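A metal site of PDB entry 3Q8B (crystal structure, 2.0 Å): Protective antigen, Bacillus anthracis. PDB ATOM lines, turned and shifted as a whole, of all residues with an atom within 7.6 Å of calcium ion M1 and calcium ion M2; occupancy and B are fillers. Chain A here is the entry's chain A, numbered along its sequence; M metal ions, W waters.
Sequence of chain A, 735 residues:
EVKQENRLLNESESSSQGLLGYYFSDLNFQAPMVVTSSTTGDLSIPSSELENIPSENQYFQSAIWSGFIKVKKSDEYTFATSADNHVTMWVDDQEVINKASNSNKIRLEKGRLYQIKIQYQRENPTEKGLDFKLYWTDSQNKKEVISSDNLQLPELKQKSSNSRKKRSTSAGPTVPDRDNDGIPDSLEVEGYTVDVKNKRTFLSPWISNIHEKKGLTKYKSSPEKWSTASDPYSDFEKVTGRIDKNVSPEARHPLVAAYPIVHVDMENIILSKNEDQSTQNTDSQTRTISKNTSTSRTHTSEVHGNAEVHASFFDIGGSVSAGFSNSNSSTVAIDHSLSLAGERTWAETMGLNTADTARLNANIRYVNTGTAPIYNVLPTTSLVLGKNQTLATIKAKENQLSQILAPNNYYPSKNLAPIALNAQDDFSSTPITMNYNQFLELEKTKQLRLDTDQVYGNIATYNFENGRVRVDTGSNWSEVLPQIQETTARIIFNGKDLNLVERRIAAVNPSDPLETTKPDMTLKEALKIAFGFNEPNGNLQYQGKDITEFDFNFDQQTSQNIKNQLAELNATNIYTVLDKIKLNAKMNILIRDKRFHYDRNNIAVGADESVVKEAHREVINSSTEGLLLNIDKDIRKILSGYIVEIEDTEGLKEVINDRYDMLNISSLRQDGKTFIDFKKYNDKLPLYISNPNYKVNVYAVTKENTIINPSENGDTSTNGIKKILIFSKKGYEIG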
ATOM      1  N   TYR A  22      30.520 -16.004   1.260  1.00  0.00           N
ATOM      2  CA  TYR A  22      29.342 -16.298   0.461  1.00  0.00           C
ATOM      3  C   TYR A  22      29.001 -15.021  -0.295  1.00  0.00           C
ATOM      4  O   TYR A  22      28.786 -13.996   0.335  1.00  0.00           O
ATOM      5  CB  TYR A  22      28.158 -16.669   1.335  1.00  0.00           C
ATOM      6  CG  TYR A  22      28.331 -17.939   2.146  1.00  0.00           C
ATOM      7  CD1 TYR A  22      29.143 -18.967   1.706  1.00  0.00           C
ATOM      8  CD2 TYR A  22      27.658 -18.125   3.353  1.00  0.00           C
ATOM      9  CE1 TYR A  22      29.311 -20.126   2.437  1.00  0.00           C
ATOM     10  CE2 TYR A  22      27.813 -19.296   4.092  1.00  0.00           C
ATOM     11  CZ  TYR A  22      28.648 -20.289   3.623  1.00  0.00           C
ATOM     12  OH  TYR A  22      28.811 -21.462   4.325  1.00  0.00           O
ATOM     13  N   PRO A 176      22.675 -19.918   6.316  1.00  0.00           N
ATOM     14  CA  PRO A 176      21.824 -20.804   5.509  1.00  0.00           C
ATOM     15  C   PRO A 176      22.592 -22.126   5.205  1.00  0.00           C
ATOM     16  O   PRO A 176      22.828 -22.461   4.040  1.00  0.00           O
ATOM     17  CB  PRO A 176      21.567 -19.985   4.235  1.00  0.00           C
ATOM     18  CG  PRO A 176      22.706 -18.941   4.187  1.00  0.00           C
ATOM     19  CD  PRO A 176      23.501 -19.036   5.472  1.00  0.00           C
ATOM     20  N   ASP A 177      22.962 -22.837   6.273  1.00  0.00           N
ATOM     21  CA  ASP A 177      23.870 -23.982   6.211  1.00  0.00           C
ATOM     22  C   ASP A 177      23.465 -24.989   7.314  1.00  0.00           C
ATOM     23  O   ASP A 177      24.127 -25.120   8.341  1.00  0.00           O
ATOM     24  CB  ASP A 177      25.315 -23.495   6.388  1.00  0.00           C
ATOM     25  CG  ASP A 177      26.360 -24.593   6.137  1.00  0.00           C
ATOM     26  OD1 ASP A 177      25.968 -25.678   5.703  1.00  0.00           O
ATOM     27  OD2 ASP A 177      27.552 -24.363   6.392  1.00  0.00           O
ATOM     28  N   ARG A 178      22.347 -25.665   7.085  1.00  0.00           N
ATOM     29  CA  ARG A 178      21.714 -26.490   8.102  1.00  0.00           C
ATOM     30  C   ARG A 178      22.680 -27.483   8.710  1.00  0.00           C
ATOM     31  O   ARG A 178      22.670 -27.700   9.910  1.00  0.00           O
ATOM     32  CB  ARG A 178      20.513 -27.240   7.515  1.00  0.00           C
ATOM     33  CG  ARG A 178      19.330 -26.337   7.217  1.00  0.00           C
ATOM     34  CD  ARG A 178      18.385 -26.951   6.214  1.00  0.00           C
ATOM     35  NE  ARG A 178      17.284 -27.626   6.864  1.00  0.00           N
ATOM     36  CZ  ARG A 178      16.283 -26.978   7.442  1.00  0.00           C
ATOM     37  NH1 ARG A 178      16.286 -25.656   7.455  1.00  0.00           N
ATOM     38  NH2 ARG A 178      15.300 -27.663   8.024  1.00  0.00           N
ATOM     39  N   ASP A 179      23.512 -28.119   7.887  1.00  0.00           N
ATOM     40  CA  ASP A 179      24.409 -29.153   8.445  1.00  0.00           C
ATOM     41  C   ASP A 179      25.805 -28.610   8.816  1.00  0.00           C
ATOM     42  O   ASP A 179      26.686 -29.362   9.222  1.00  0.00           O
ATOM     43  CB  ASP A 179      24.524 -30.350   7.478  1.00  0.00           C
ATOM     44  CG  ASP A 179      25.030 -29.945   6.096  1.00  0.00           C
ATOM     45  OD1 ASP A 179      25.663 -28.883   5.973  1.00  0.00           O
ATOM     46  OD2 ASP A 179      24.809 -30.688   5.131  1.00  0.00           O
ATOM     47  N   ASN A 180      26.016 -27.315   8.663  1.00  0.00           N
ATOM     48  CA  ASN A 180      27.307 -26.699   9.003  1.00  0.00           C
ATOM     49  C   ASN A 180      28.503 -27.277   8.239  1.00  0.00           C
ATOM     50  O   ASN A 180      29.639 -27.230   8.752  1.00  0.00           O
ATOM     51  CB  ASN A 180      27.544 -26.776  10.533  1.00  0.00           C
ATOM     52  CG  ASN A 180      28.730 -25.896  11.027  1.00  0.00           C
ATOM     53  OD1 ASN A 180      29.388 -26.251  12.000  1.00  0.00           O
ATOM     54  ND2 ASN A 180      29.001 -24.786  10.363  1.00  0.00           N
ATOM     55  N   ASP A 181      28.328 -27.777   6.995  1.00  0.00           N
ATOM     56  CA  ASP A 181      29.533 -28.233   6.308  1.00  0.00           C
ATOM     57  C   ASP A 181      30.196 -27.053   5.577  1.00  0.00           C
ATOM     58  O   ASP A 181      31.336 -27.150   5.105  1.00  0.00           O
ATOM     59  CB  ASP A 181      29.300 -29.475   5.394  1.00  0.00           C
ATOM     60  CG  ASP A 181      28.263 -29.226   4.313  1.00  0.00           C
ATOM     61  OD1 ASP A 181      28.063 -28.063   3.894  1.00  0.00           O
ATOM     62  OD2 ASP A 181      27.647 -30.196   3.842  1.00  0.00           O
ATOM     63  N   GLY A 182      29.504 -25.932   5.513  1.00  0.00           N
ATOM     64  CA  GLY A 182      29.979 -24.781   4.756  1.00  0.00           C
ATOM     65  C   GLY A 182      29.310 -24.528   3.402  1.00  0.00           C
ATOM     66  O   GLY A 182      29.405 -23.439   2.859  1.00  0.00           O
ATOM     67  N   ILE A 183      28.679 -25.537   2.803  1.00  0.00           N
ATOM     68  CA  ILE A 183      27.986 -25.340   1.518  1.00  0.00           C
ATOM     69  C   ILE A 183      26.531 -24.922   1.784  1.00  0.00           C
ATOM     70  O   ILE A 183      25.811 -25.627   2.463  1.00  0.00           O
ATOM     71  CB  ILE A 183      27.970 -26.649   0.654  1.00  0.00           C
ATOM     72  CG1 ILE A 183      29.388 -27.236   0.555  1.00  0.00           C
ATOM     73  CG2 ILE A 183      27.354 -26.373  -0.726  1.00  0.00           C
ATOM     74  CD1 ILE A 183      29.496 -28.623  -0.184  1.00  0.00           C
ATOM     75  N   PRO A 184      26.100 -23.775   1.241  1.00  0.00           N
ATOM     76  CA  PRO A 184      24.721 -23.326   1.458  1.00  0.00           C
ATOM     77  C   PRO A 184      23.699 -24.379   1.061  1.00  0.00           C
ATOM     78  O   PRO A 184      23.887 -25.093   0.044  1.00  0.00           O
ATOM     79  CB  PRO A 184      24.574 -22.089   0.544  1.00  0.00           C
ATOM     80  CG  PRO A 184      25.963 -21.586   0.374  1.00  0.00           C
ATOM     81  CD  PRO A 184      26.867 -22.814   0.423  1.00  0.00           C
ATOM     82  N   ASP A 185      22.604 -24.446   1.812  1.00  0.00           N
ATOM     83  CA  ASP A 185      21.597 -25.467   1.601  1.00  0.00           C
ATOM     84  C   ASP A 185      21.204 -25.534   0.137  1.00  0.00           C
ATOM     85  O   ASP A 185      21.077 -26.624  -0.437  1.00  0.00           O
ATOM     86  CB  ASP A 185      20.330 -25.211   2.418  1.00  0.00           C
ATOM     87  CG  ASP A 185      20.600 -25.026   3.891  1.00  0.00           C
ATOM     88  OD1 ASP A 185      21.674 -25.417   4.371  1.00  0.00           O
ATOM     89  OD2 ASP A 185      19.716 -24.461   4.575  1.00  0.00           O
ATOM     90  N   SER A 186      20.994 -24.372  -0.466  1.00  0.00           N
ATOM     91  CA  SER A 186      20.355 -24.337  -1.788  1.00  0.00           C
ATOM     92  C   SER A 186      21.293 -24.854  -2.861  1.00  0.00           C
ATOM     93  O   SER A 186      20.826 -25.425  -3.836  1.00  0.00           O
ATOM     94  CB  SER A 186      19.858 -22.919  -2.150  1.00  0.00           C
ATOM     95  OG  SER A 186      20.953 -22.028  -2.374  1.00  0.00           O
ATOM     96  N   GLU A 188      23.588 -27.255  -2.398  1.00  0.00           N
ATOM     97  CA  GLU A 188      23.677 -28.703  -2.217  1.00  0.00           C
ATOM     98  C   GLU A 188      22.507 -29.392  -2.877  1.00  0.00           C
ATOM     99  O   GLU A 188      22.641 -30.447  -3.510  1.00  0.00           O
ATOM    100  CB  GLU A 188      23.699 -29.043  -0.745  1.00  0.00           C
ATOM    101  CG  GLU A 188      25.007 -28.722  -0.128  1.00  0.00           C
ATOM    102  CD  GLU A 188      25.268 -29.583   1.067  1.00  0.00           C
ATOM    103  OE1 GLU A 188      25.567 -30.809   0.885  1.00  0.00           O
ATOM    104  OE2 GLU A 188      25.139 -29.028   2.178  1.00  0.00           O
ATOM    105  N   TYR A 192      26.011 -28.011  -7.872  1.00  0.00           N
ATOM    106  CA  TYR A 192      27.157 -27.113  -7.864  1.00  0.00           C
ATOM    107  C   TYR A 192      28.387 -27.743  -8.484  1.00  0.00           C
ATOM    108  O   TYR A 192      28.458 -28.967  -8.685  1.00  0.00           O
ATOM    109  CB  TYR A 192      27.485 -26.687  -6.419  1.00  0.00           C
ATOM    110  CG  TYR A 192      27.772 -27.822  -5.444  1.00  0.00           C
ATOM    111  CD1 TYR A 192      26.730 -28.567  -4.901  1.00  0.00           C
ATOM    112  CD2 TYR A 192      29.078 -28.096  -5.021  1.00  0.00           C
ATOM    113  CE1 TYR A 192      26.976 -29.570  -3.986  1.00  0.00           C
ATOM    114  CE2 TYR A 192      29.344 -29.122  -4.109  1.00  0.00           C
ATOM    115  CZ  TYR A 192      28.278 -29.859  -3.591  1.00  0.00           C
ATOM    116  OH  TYR A 192      28.474 -30.867  -2.666  1.00  0.00           O
ATOM    117  N   SER A 221      24.426 -32.923  -3.032  1.00  0.00           N
ATOM    118  CA  SER A 221      24.633 -33.538  -1.700  1.00  0.00           C
ATOM    119  C   SER A 221      23.476 -33.202  -0.736  1.00  0.00           C
ATOM    120  O   SER A 221      22.691 -32.298  -1.030  1.00  0.00           O
ATOM    121  CB  SER A 221      25.982 -33.139  -1.118  1.00  0.00           C
ATOM    122  OG  SER A 221      26.341 -31.791  -1.412  1.00  0.00           O
ATOM    123  N   SER A 222      23.325 -33.908   0.377  1.00  0.00           N
ATOM    124  CA  SER A 222      22.264 -33.539   1.326  1.00  0.00           C
ATOM    125  C   SER A 222      22.620 -32.269   2.094  1.00  0.00           C
ATOM    126  O   SER A 222      23.709 -32.154   2.586  1.00  0.00           O
ATOM    127  CB  SER A 222      21.979 -34.632   2.346  1.00  0.00           C
ATOM    128  OG  SER A 222      21.037 -34.119   3.289  1.00  0.00           O
ATOM    129  N   PRO A 223      21.685 -31.311   2.191  1.00  0.00           N
ATOM    130  CA  PRO A 223      21.987 -30.087   2.949  1.00  0.00           C
ATOM    131  C   PRO A 223      21.921 -30.280   4.453  1.00  0.00           C
ATOM    132  O   PRO A 223      22.273 -29.387   5.228  1.00  0.00           O
ATOM    133  CB  PRO A 223      20.893 -29.088   2.480  1.00  0.00           C
ATOM    134  CG  PRO A 223      19.746 -29.942   2.063  1.00  0.00           C
ATOM    135  CD  PRO A 223      20.368 -31.259   1.518  1.00  0.00           C
ATOM    136  N   GLU A 224      21.453 -31.452   4.836  1.00  0.00           N
ATOM    137  CA  GLU A 224      21.308 -31.809   6.236  1.00  0.00           C
ATOM    138  C   GLU A 224      22.238 -32.939   6.705  1.00  0.00           C
ATOM    139  O   GLU A 224      22.178 -33.329   7.857  1.00  0.00           O
ATOM    140  CB  GLU A 224      19.850 -32.156   6.506  1.00  0.00           C
ATOM    141  CG  GLU A 224      18.933 -30.906   6.258  1.00  0.00           C
ATOM    142  CD  GLU A 224      17.473 -31.244   6.183  1.00  0.00           C
ATOM    143  OE1 GLU A 224      16.724 -30.516   5.475  1.00  0.00           O
ATOM    144  OE2 GLU A 224      17.062 -32.234   6.829  1.00  0.00           O
ATOM    145  N   LYS A 225      23.079 -33.467   5.819  1.00  0.00           N
ATOM    146  CA  LYS A 225      24.156 -34.369   6.237  1.00  0.00           C
ATOM    147  C   LYS A 225      25.492 -33.707   6.005  1.00  0.00           C
ATOM    148  O   LYS A 225      25.845 -33.436   4.873  1.00  0.00           O
ATOM    149  CB  LYS A 225      24.128 -35.665   5.397  1.00  0.00           C
ATOM    150  CG  LYS A 225      22.923 -36.587   5.641  1.00  0.00           C
ATOM    151  CD  LYS A 225      22.952 -37.780   4.686  1.00  0.00           C
ATOM    152  CE  LYS A 225      23.871 -38.891   5.143  1.00  0.00           C
ATOM    153  NZ  LYS A 225      23.227 -39.576   6.252  1.00  0.00           N
ATOM    154  N   TRP A 226      26.274 -33.522   7.069  1.00  0.00           N
ATOM    155  CA  TRP A 226      27.565 -32.902   6.988  1.00  0.00           C
ATOM    156  C   TRP A 226      28.474 -33.721   6.013  1.00  0.00           C
ATOM    157  O   TRP A 226      29.259 -33.163   5.244  1.00  0.00           O
ATOM    158  CB  TRP A 226      28.113 -32.815   8.416  1.00  0.00           C
ATOM    159  CG  TRP A 226      29.483 -32.322   8.556  1.00  0.00           C
ATOM    160  CD1 TRP A 226      29.864 -31.028   8.688  1.00  0.00           C
ATOM    161  CD2 TRP A 226      30.683 -33.106   8.629  1.00  0.00           C
ATOM    162  NE1 TRP A 226      31.230 -30.952   8.822  1.00  0.00           N
ATOM    163  CE2 TRP A 226      31.754 -32.211   8.801  1.00  0.00           C
ATOM    164  CE3 TRP A 226      30.947 -34.495   8.557  1.00  0.00           C
ATOM    165  CZ2 TRP A 226      33.094 -32.648   8.896  1.00  0.00           C
ATOM    166  CZ3 TRP A 226      32.274 -34.916   8.654  1.00  0.00           C
ATOM    167  CH2 TRP A 226      33.333 -33.992   8.824  1.00  0.00           C
ATOM    168  N   SER A 227      28.326 -35.043   6.060  1.00  0.00           N
ATOM    169  CA  SER A 227      28.913 -35.942   5.059  1.00  0.00           C
ATOM    170  C   SER A 227      27.759 -36.735   4.508  1.00  0.00           C
ATOM    171  O   SER A 227      27.104 -37.482   5.249  1.00  0.00           O
ATOM    172  CB  SER A 227      29.943 -36.894   5.686  1.00  0.00           C
ATOM    173  OG  SER A 227      30.354 -37.899   4.728  1.00  0.00           O
ATOM    174  N   THR A 228      27.479 -36.523   3.228  1.00  0.00           N
ATOM    175  CA  THR A 228      26.324 -37.149   2.613  1.00  0.00           C
ATOM    176  C   THR A 228      26.520 -38.675   2.515  1.00  0.00           C
ATOM    177  O   THR A 228      25.566 -39.443   2.618  1.00  0.00           O
ATOM    178  CB  THR A 228      26.036 -36.482   1.256  1.00  0.00           C
ATOM    179  OG1 THR A 228      25.624 -35.122   1.506  1.00  0.00           O
ATOM    180  CG2 THR A 228      24.948 -37.220   0.487  1.00  0.00           C
ATOM    181  N   SER A 234      33.678 -34.107   5.388  1.00  0.00           N
ATOM    182  CA  SER A 234      32.495 -33.343   5.003  1.00  0.00           C
ATOM    183  C   SER A 234      32.347 -33.095   3.483  1.00  0.00           C
ATOM    184  O   SER A 234      33.327 -33.141   2.719  1.00  0.00           O
ATOM    185  CB  SER A 234      32.467 -31.994   5.764  1.00  0.00           C
ATOM    186  OG  SER A 234      32.804 -30.926   4.906  1.00  0.00           O
ATOM    187  N   ASP A 235      31.133 -32.830   3.025  1.00  0.00           N
ATOM    188  CA  ASP A 235      30.911 -32.643   1.584  1.00  0.00           C
ATOM    189  C   ASP A 235      31.782 -31.480   1.105  1.00  0.00           C
ATOM    190  O   ASP A 235      32.260 -31.434  -0.021  1.00  0.00           O
ATOM    191  CB  ASP A 235      29.436 -32.318   1.305  1.00  0.00           C
ATOM    192  CG  ASP A 235      28.513 -33.395   1.805  1.00  0.00           C
ATOM    193  OD1 ASP A 235      28.935 -34.568   1.893  1.00  0.00           O
ATOM    194  OD2 ASP A 235      27.351 -33.094   2.070  1.00  0.00           O
ATOM    195  N   PHE A 236      31.969 -30.503   1.982  1.00  0.00           N
ATOM    196  CA  PHE A 236      32.765 -29.328   1.642  1.00  0.00           C
ATOM    197  C   PHE A 236      34.282 -29.617   1.684  1.00  0.00           C
ATOM    198  O   PHE A 236      35.022 -29.181   0.809  1.00  0.00           O
ATOM    199  CB  PHE A 236      32.375 -28.169   2.575  1.00  0.00           C
ATOM    200  CG  PHE A 236      33.191 -26.927   2.388  1.00  0.00           C
ATOM    201  CD1 PHE A 236      32.900 -26.031   1.363  1.00  0.00           C
ATOM    202  CD2 PHE A 236      34.223 -26.625   3.278  1.00  0.00           C
ATOM    203  CE1 PHE A 236      33.657 -24.844   1.214  1.00  0.00           C
ATOM    204  CE2 PHE A 236      34.979 -25.452   3.132  1.00  0.00           C
ATOM    205  CZ  PHE A 236      34.695 -24.564   2.106  1.00  0.00           C
ATOM    206  N   PRO A 254      31.054 -36.176  -2.990  1.00  0.00           N
ATOM    207  CA  PRO A 254      30.262 -36.255  -1.762  1.00  0.00           C
ATOM    208  C   PRO A 254      29.331 -37.460  -1.747  1.00  0.00           C
ATOM    209  O   PRO A 254      28.811 -37.749  -0.688  1.00  0.00           O
ATOM    210  CB  PRO A 254      29.461 -34.942  -1.763  1.00  0.00           C
ATOM    211  CG  PRO A 254      30.266 -33.991  -2.560  1.00  0.00           C
ATOM    212  CD  PRO A 254      30.984 -34.847  -3.625  1.00  0.00           C
HETATM  213 CA    CA M   1      25.583 -27.483   3.961  1.00  0.00          CA
HETATM  214 CA    CA M   2      26.010 -31.589   3.193  1.00  0.00          CA
HETATM  215  O   HOH W   1      23.244 -27.313   4.283  1.00  0.00           O
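Calcium ion M2 is bound by OD2 of Asp 181 (2.2 Å), OD2 of Asp 235 (2.3 Å), O of Ser 222 (2.4 Å), OD2 of Asp 179 (2.5 Å), OE1 of Glu 188 (2.5 Å), O of Lys 225 (2.5 Å) and OE2 of Glu 188 (2.9 Å). Calcium ion M2 has seven donor atoms within binding distance.
Merely in contact with calcium ion M2: Thr 228. Seven residues have an atom within 4 Å of calcium ion M2: Asp 179, Asp 181, Glu 188, Ser 222, Lys 225, Thr 228 and Asp 235. The nearest printed residue that does not touch calcium ion M2 is Trp 226 (4.2 Å).
Of the 26 residues printed, 5 come within 4 Å of calcium ion M1. Along chain A the residues within 4 Å of calcium ion M1 span positions 177 to 188. The nearest printed residue that does not touch calcium ion M1 is Pro 223 (4.02 Å).
Calcium ion M1 is bound by water W1, the backbone carbonyl oxygen (O) of Ile 183, the side-chain carboxylate (OE2) of Glu 188, the side-chain carboxylate (OD1) of Asp 179, the side-chain carboxylate (OD1) of Asp 177 and the side-chain carboxylate (OD1) of Asp 181. Calcium ion M1 has six donor atoms within binding distance.
Water W1 lies within hydrogen-bond range of the side-chain carboxylate (OD1) of Asp 185, the backbone carbonyl oxygen (O) of Pro 223 and the backbone NH (N) of Arg 178.
The backbone NH of Glu 224 lies close to the side-chain hydroxyl of Ser 222 (3.1 Å). The side-chain carboxylate (OD2) of Asp 177 is in hydrogen-bond range of the backbone NH (N) of Gly 182 (2.7 Å). The backbone NH (N) of Asp 235 is in hydrogen-bond range of the backbone carbonyl oxygen (O) of Trp 226 (2.9 Å). The backbone carbonyl oxygen of Glu 188 sits at hydrogen-bond distance from the backbone NH of Ser 221 (3.1 Å). The backbone carbonyl oxygen (O) of Pro 223 lies close to the backbone NH (N) of Asp 179, 3.2 Å away. OD1 of Asp 177 sits close to N of Asn 180 (3.4 Å). The side-chain carboxylate (OD1) of Asp 185 lies close to the backbone NH (N) of Asp 177, 3.5 Å away. OG1 of Thr 228 sits at hydrogen-bond distance from N of Ser 222, at 2.8 Å.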
